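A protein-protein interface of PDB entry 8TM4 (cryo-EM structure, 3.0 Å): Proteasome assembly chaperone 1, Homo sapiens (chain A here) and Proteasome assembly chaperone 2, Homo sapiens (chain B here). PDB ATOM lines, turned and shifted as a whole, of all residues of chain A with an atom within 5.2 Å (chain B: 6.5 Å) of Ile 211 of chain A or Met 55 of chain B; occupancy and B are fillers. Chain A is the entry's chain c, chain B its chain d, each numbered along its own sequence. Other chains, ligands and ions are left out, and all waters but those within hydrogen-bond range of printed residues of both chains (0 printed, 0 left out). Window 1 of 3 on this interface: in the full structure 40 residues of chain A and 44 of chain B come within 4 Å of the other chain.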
ATOM      1  N   LEU A 206      30.245  -5.552  29.422  1.00  0.00           N
ATOM      2  CA  LEU A 206      30.409  -6.481  28.267  1.00  0.00           C
ATOM      3  C   LEU A 206      31.894  -6.618  27.911  1.00  0.00           C
ATOM      4  O   LEU A 206      32.699  -5.796  28.385  1.00  0.00           O
ATOM      5  CB  LEU A 206      29.615  -5.978  27.054  1.00  0.00           C
ATOM      6  CG  LEU A 206      28.180  -6.490  26.920  1.00  0.00           C
ATOM      7  CD1 LEU A 206      27.487  -5.833  25.735  1.00  0.00           C
ATOM      8  CD2 LEU A 206      28.139  -8.010  26.801  1.00  0.00           C
ATOM      9  N   GLN A 208      35.052  -6.761  24.871  1.00  0.00           N
ATOM     10  CA  GLN A 208      35.402  -5.961  23.666  1.00  0.00           C
ATOM     11  C   GLN A 208      34.625  -6.514  22.461  1.00  0.00           C
ATOM     12  O   GLN A 208      33.840  -5.731  21.911  1.00  0.00           O
ATOM     13  CB  GLN A 208      36.920  -5.899  23.448  1.00  0.00           C
ATOM     14  CG  GLN A 208      37.709  -5.341  24.629  1.00  0.00           C
ATOM     15  CD  GLN A 208      37.050  -4.145  25.275  1.00  0.00           C
ATOM     16  OE1 GLN A 208      36.980  -3.068  24.692  1.00  0.00           O
ATOM     17  NE2 GLN A 208      36.543  -4.324  26.485  1.00  0.00           N
ATOM     18  N   PRO A 209      34.740  -7.798  22.035  1.00  0.00           N
ATOM     19  CA  PRO A 209      33.979  -8.293  20.879  1.00  0.00           C
ATOM     20  C   PRO A 209      32.473  -8.017  21.003  1.00  0.00           C
ATOM     21  O   PRO A 209      31.858  -7.688  20.005  1.00  0.00           O
ATOM     22  CB  PRO A 209      34.235  -9.809  20.837  1.00  0.00           C
ATOM     23  CG  PRO A 209      34.852 -10.134  22.179  1.00  0.00           C
ATOM     24  CD  PRO A 209      35.576  -8.869  22.587  1.00  0.00           C
ATOM     25  N   ASN A 210      31.926  -8.151  22.215  1.00  0.00           N
ATOM     26  CA  ASN A 210      30.477  -7.985  22.508  1.00  0.00           C
ATOM     27  C   ASN A 210      30.035  -6.555  22.174  1.00  0.00           C
ATOM     28  O   ASN A 210      30.716  -5.610  22.623  1.00  0.00           O
ATOM     29  CB  ASN A 210      30.134  -8.288  23.966  1.00  0.00           C
ATOM     30  CG  ASN A 210      29.879  -9.757  24.227  1.00  0.00           C
ATOM     31  OD1 ASN A 210      28.733 -10.192  24.236  1.00  0.00           O
ATOM     32  ND2 ASN A 210      30.934 -10.528  24.429  1.00  0.00           N
ATOM     33  N   ILE A 211      28.928  -6.416  21.434  1.00  0.00           N
ATOM     34  CA  ILE A 211      28.231  -5.124  21.149  1.00  0.00           C
ATOM     35  C   ILE A 211      26.726  -5.324  21.367  1.00  0.00           C
ATOM     36  O   ILE A 211      26.305  -6.489  21.512  1.00  0.00           O
ATOM     37  CB  ILE A 211      28.556  -4.606  19.728  1.00  0.00           C
ATOM     38  CG1 ILE A 211      28.400  -5.689  18.655  1.00  0.00           C
ATOM     39  CG2 ILE A 211      29.941  -3.978  19.698  1.00  0.00           C
ATOM     40  CD1 ILE A 211      28.269  -5.156  17.242  1.00  0.00           C
ATOM     41  N   VAL A 212      25.966  -4.224  21.404  1.00  0.00           N
ATOM     42  CA  VAL A 212      24.473  -4.186  21.417  1.00  0.00           C
ATOM     43  C   VAL A 212      24.041  -3.470  20.134  1.00  0.00           C
ATOM     44  O   VAL A 212      24.914  -2.858  19.500  1.00  0.00           O
ATOM     45  CB  VAL A 212      23.929  -3.470  22.670  1.00  0.00           C
ATOM     46  CG1 VAL A 212      22.440  -3.710  22.873  1.00  0.00           C
ATOM     47  CG2 VAL A 212      24.704  -3.836  23.930  1.00  0.00           C
ATOM     48  N   HIS A 213      22.760  -3.557  19.761  1.00  0.00           N
ATOM     49  CA  HIS A 213      22.091  -2.643  18.797  1.00  0.00           C
ATOM     50  C   HIS A 213      20.600  -2.552  19.144  1.00  0.00           C
ATOM     51  O   HIS A 213      20.200  -3.195  20.135  1.00  0.00           O
ATOM     52  CB  HIS A 213      22.373  -3.086  17.353  1.00  0.00           C
ATOM     53  CG  HIS A 213      21.739  -4.378  16.964  1.00  0.00           C
ATOM     54  ND1 HIS A 213      20.706  -4.447  16.051  1.00  0.00           N
ATOM     55  CD2 HIS A 213      21.996  -5.647  17.345  1.00  0.00           C
ATOM     56  CE1 HIS A 213      20.348  -5.705  15.892  1.00  0.00           C
ATOM     57  NE2 HIS A 213      21.123  -6.461  16.676  1.00  0.00           N
ATOM     58  N   ALA A 217      20.498   0.363  22.764  1.00  0.00           N
ATOM     59  CA  ALA A 217      21.736   0.942  22.198  1.00  0.00           C
ATOM     60  C   ALA A 217      21.482   2.402  21.810  1.00  0.00           C
ATOM     61  O   ALA A 217      22.299   3.252  22.185  1.00  0.00           O
ATOM     62  CB  ALA A 217      22.201   0.126  21.017  1.00  0.00           C
ATOM     63  N   SER A 221      23.497   5.488  23.493  1.00  0.00           N
ATOM     64  CA  SER A 221      24.371   6.180  22.509  1.00  0.00           C
ATOM     65  C   SER A 221      24.000   7.665  22.455  1.00  0.00           C
ATOM     66  O   SER A 221      24.919   8.503  22.533  1.00  0.00           O
ATOM     67  CB  SER A 221      24.315   5.534  21.142  1.00  0.00           C
ATOM     68  OG  SER A 221      23.029   5.660  20.559  1.00  0.00           O
ATOM     69  N   TYR A 236      21.353 -11.664  29.299  1.00  0.00           N
ATOM     70  CA  TYR A 236      21.728 -12.750  28.352  1.00  0.00           C
ATOM     71  C   TYR A 236      21.253 -14.100  28.907  1.00  0.00           C
ATOM     72  O   TYR A 236      22.069 -14.822  29.515  1.00  0.00           O
ATOM     73  CB  TYR A 236      23.241 -12.746  28.101  1.00  0.00           C
ATOM     74  CG  TYR A 236      23.751 -11.567  27.309  1.00  0.00           C
ATOM     75  CD1 TYR A 236      23.667 -11.558  25.928  1.00  0.00           C
ATOM     76  CD2 TYR A 236      24.320 -10.466  27.927  1.00  0.00           C
ATOM     77  CE1 TYR A 236      24.122 -10.489  25.179  1.00  0.00           C
ATOM     78  CE2 TYR A 236      24.781  -9.385  27.191  1.00  0.00           C
ATOM     79  CZ  TYR A 236      24.677  -9.396  25.813  1.00  0.00           C
ATOM     80  OH  TYR A 236      25.118  -8.345  25.064  1.00  0.00           O
ATOM     81  N   VAL B  53      22.601   2.602  11.868  1.00  0.00           N
ATOM     82  CA  VAL B  53      21.709   1.848  12.799  1.00  0.00           C
ATOM     83  C   VAL B  53      22.372   1.863  14.180  1.00  0.00           C
ATOM     84  O   VAL B  53      23.516   1.390  14.271  1.00  0.00           O
ATOM     85  CB  VAL B  53      21.447   0.412  12.297  1.00  0.00           C
ATOM     86  CG1 VAL B  53      20.716  -0.442  13.326  1.00  0.00           C
ATOM     87  CG2 VAL B  53      20.691   0.412  10.977  1.00  0.00           C
ATOM     88  N   PRO B  54      21.738   2.387  15.255  1.00  0.00           N
ATOM     89  CA  PRO B  54      22.464   2.684  16.488  1.00  0.00           C
ATOM     90  C   PRO B  54      23.031   1.402  17.115  1.00  0.00           C
ATOM     91  O   PRO B  54      22.357   0.390  17.077  1.00  0.00           O
ATOM     92  CB  PRO B  54      21.427   3.323  17.419  1.00  0.00           C
ATOM     93  CG  PRO B  54      20.099   2.851  16.880  1.00  0.00           C
ATOM     94  CD  PRO B  54      20.305   2.660  15.392  1.00  0.00           C
ATOM     95  N   MET B  55      24.244   1.485  17.665  1.00  0.00           N
ATOM     96  CA  MET B  55      24.918   0.390  18.409  1.00  0.00           C
ATOM     97  C   MET B  55      25.782   1.017  19.504  1.00  0.00           C
ATOM     98  O   MET B  55      26.120   2.213  19.377  1.00  0.00           O
ATOM     99  CB  MET B  55      25.787  -0.480  17.491  1.00  0.00           C
ATOM    100  CG  MET B  55      26.943   0.243  16.829  1.00  0.00           C
ATOM    101  SD  MET B  55      28.466   0.236  17.810  1.00  0.00           S
ATOM    102  CE  MET B  55      29.032  -1.441  17.532  1.00  0.00           C
ATOM    103  N   VAL B  56      26.094   0.239  20.543  1.00  0.00           N
ATOM    104  CA  VAL B  56      27.090   0.588  21.596  1.00  0.00           C
ATOM    105  C   VAL B  56      28.047  -0.603  21.731  1.00  0.00           C
ATOM    106  O   VAL B  56      27.934  -1.523  20.906  1.00  0.00           O
ATOM    107  CB  VAL B  56      26.394   0.983  22.918  1.00  0.00           C
ATOM    108  CG1 VAL B  56      25.549   2.238  22.734  1.00  0.00           C
ATOM    109  CG2 VAL B  56      25.554  -0.145  23.504  1.00  0.00           C
ATOM    110  N   GLY B  57      28.975  -0.568  22.695  1.00  0.00           N
ATOM    111  CA  GLY B  57      29.982  -1.620  22.935  1.00  0.00           C
ATOM    112  C   GLY B  57      30.985  -1.142  23.965  1.00  0.00           C
ATOM    113  O   GLY B  57      30.572  -0.415  24.875  1.00  0.00           O
ATOM    114  N   ASN B  58      32.260  -1.502  23.806  1.00  0.00           N
ATOM    115  CA  ASN B  58      33.410  -0.837  24.474  1.00  0.00           C
ATOM    116  C   ASN B  58      34.355  -0.321  23.387  1.00  0.00           C
ATOM    117  O   ASN B  58      34.256  -0.818  22.272  1.00  0.00           O
ATOM    118  CB  ASN B  58      34.117  -1.788  25.437  1.00  0.00           C
ATOM    119  CG  ASN B  58      33.237  -2.204  26.596  1.00  0.00           C
ATOM    120  OD1 ASN B  58      32.776  -1.361  27.363  1.00  0.00           O
ATOM    121  ND2 ASN B  58      32.998  -3.496  26.739  1.00  0.00           N
ATOM    122  N   SER B  72      31.671   2.354  22.975  1.00  0.00           N
ATOM    123  CA  SER B  72      31.574   2.403  21.491  1.00  0.00           C
ATOM    124  C   SER B  72      30.275   3.114  21.088  1.00  0.00           C
ATOM    125  O   SER B  72      29.315   3.053  21.877  1.00  0.00           O
ATOM    126  CB  SER B  72      31.670   1.015  20.893  1.00  0.00           C
ATOM    127  OG  SER B  72      31.129   0.977  19.583  1.00  0.00           O
ATOM    128  N   ILE B  73      30.269   3.800  19.936  1.00  0.00           N
ATOM    129  CA  ILE B  73      29.089   4.513  19.353  1.00  0.00           C
ATOM    130  C   ILE B  73      29.062   4.234  17.844  1.00  0.00           C
ATOM    131  O   ILE B  73      30.151   4.136  17.254  1.00  0.00           O
ATOM    132  CB  ILE B  73      29.147   6.026  19.674  1.00  0.00           C
ATOM    133  CG1 ILE B  73      29.144   6.313  21.181  1.00  0.00           C
ATOM    134  CG2 ILE B  73      28.040   6.793  18.964  1.00  0.00           C
ATOM    135  CD1 ILE B  73      27.829   6.038  21.871  1.00  0.00           C
ATOM    136  N   ASN B  74      27.868   4.101  17.251  1.00  0.00           N
ATOM    137  CA  ASN B  74      27.678   3.800  15.804  1.00  0.00           C
ATOM    138  C   ASN B  74      28.617   4.681  14.970  1.00  0.00           C
ATOM    139  O   ASN B  74      29.367   4.118  14.157  1.00  0.00           O
ATOM    140  CB  ASN B  74      26.220   3.922  15.338  1.00  0.00           C
ATOM    141  CG  ASN B  74      25.569   5.270  15.575  1.00  0.00           C
ATOM    142  OD1 ASN B  74      25.914   5.993  16.507  1.00  0.00           O
ATOM    143  ND2 ASN B  74      24.595   5.605  14.746  1.00  0.00           N
ATOM    144  N   ALA B  75      28.576   5.999  15.178  1.00  0.00           N
ATOM    145  CA  ALA B  75      29.378   7.013  14.457  1.00  0.00           C
ATOM    146  C   ALA B  75      30.342   7.683  15.444  1.00  0.00           C
ATOM    147  O   ALA B  75      29.915   8.618  16.145  1.00  0.00           O
ATOM    148  CB  ALA B  75      28.459   8.008  13.794  1.00  0.00           C
ATOM    149  N   ARG B  91      30.448   1.867  12.711  1.00  0.00           N
ATOM    150  CA  ARG B  91      30.470   0.585  13.464  1.00  0.00           C
ATOM    151  C   ARG B  91      29.200  -0.199  13.130  1.00  0.00           C
ATOM    152  O   ARG B  91      28.807  -1.065  13.935  1.00  0.00           O
ATOM    153  CB  ARG B  91      30.545   0.849  14.970  1.00  0.00           C
ATOM    154  CG  ARG B  91      31.778   1.621  15.408  1.00  0.00           C
ATOM    155  CD  ARG B  91      32.853   0.720  15.985  1.00  0.00           C
ATOM    156  NE  ARG B  91      34.027   1.493  16.365  1.00  0.00           N
ATOM    157  CZ  ARG B  91      34.134   2.286  17.434  1.00  0.00           C
ATOM    158  NH1 ARG B  91      33.136   2.441  18.290  1.00  0.00           N
ATOM    159  NH2 ARG B  91      35.262   2.937  17.651  1.00  0.00           N
ATOM    160  N   SER B  92      28.562   0.134  12.006  1.00  0.00           N
ATOM    161  CA  SER B  92      27.103  -0.021  11.805  1.00  0.00           C
ATOM    162  C   SER B  92      26.755  -0.228  10.328  1.00  0.00           C
ATOM    163  O   SER B  92      27.576   0.117   9.454  1.00  0.00           O
ATOM    164  CB  SER B  92      26.373   1.157  12.389  1.00  0.00           C
ATOM    165  OG  SER B  92      26.332   1.058  13.801  1.00  0.00           O
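The side-chain amide nitrogen (ND2) of Asn 58 of chain B sits at hydrogen-bond distance from the backbone carbonyl oxygen (O) of Leu 206 of chain A (2.8 Å).
O of Val 56 of chain B sits at hydrogen-bond distance from N of Val 212 of chain A, at 3.4 Å.
The backbone carbonyl oxygen of Ala 217 of chain A is in hydrogen-bond range of the side-chain hydroxyl of Ser 221 of chain A, 3.0 Å away.
OG of Ser 72 of chain B lies within hydrogen-bond range of SD of Met 55 of chain B (3.3 Å).
The backbone carbonyl oxygen (O) of Met 55 of chain B is in hydrogen-bond range of the backbone NH (N) of Asn 74 of chain B (3.3 Å).
OE1 of Gln 208 of chain A touches CB of Asn 58 of chain B (3.2 Å).
Met 55 of chain B touches Ile 211 of chain A.
Ile 211 of chain A touches Val 56 of chain B.
Val 212 of chain A touches Met 55 of chain B (O to CB, 3.2 Å).
CB of His 213 of chain A touches O of Pro 54 of chain B, 3.5 Å away.
Ala 217 of chain A touches Pro 54 of chain B (CB to O, 3.95 Å).
Ala 217 of chain A touches Met 55 of chain B.
Ala 217 of chain A touches Val 56 of chain B.
Ser 221 of chain A touches Val 56 of chain B (CB to CG1, 3.9 Å).
Ser 221 of chain A touches Ile 73 of chain B.
Printed residues of chain B within 4 Å of Ile 211 of chain A: Met 55 (3.5 Å) and Val 56 (3.4 Å).
Of chain A, only Ile 211, Val 212 and Ala 217 come within 4 Å of Met 55 of chain B.
Printed residues of chain B within 4 Å of Val 212 of chain A: Met 55 (3.2 Å) and Val 56 (3.4 Å).
Printed residues of chain B within 4 Å of His 213 of chain A: Pro 54.
Of the printed residues of chain A, Asn 58 of chain B touches Leu 206 (2.8 Å) and Gln 208 (3.2 Å).
Of the printed residues of chain B, Gln 208 of chain A touches Asn 58 (3.2 Å).
Pro 209 of chain A touches none of the printed residues of chain B.
The nearest printed residue of chain B that does not touch Ile 211 of chain A is Gly 57 of chain B (4.005 Å).
Hydrophobic or aromatic side chains of chain A within 4 Å of the printed part of chain B: Ile 211, Val 212, His 213 and Ala 217.
Hydrophobic or aromatic side chains of chain B that line the printed part of chain A: Met 55, Val 56 and Ile 73.
Among the printed residues, 12 pairs touch across the chains.
Among the printed residues, no Asp or Glu carboxylate lies within 4 Å of a Lys or Arg side-chain nitrogen of the other chain.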
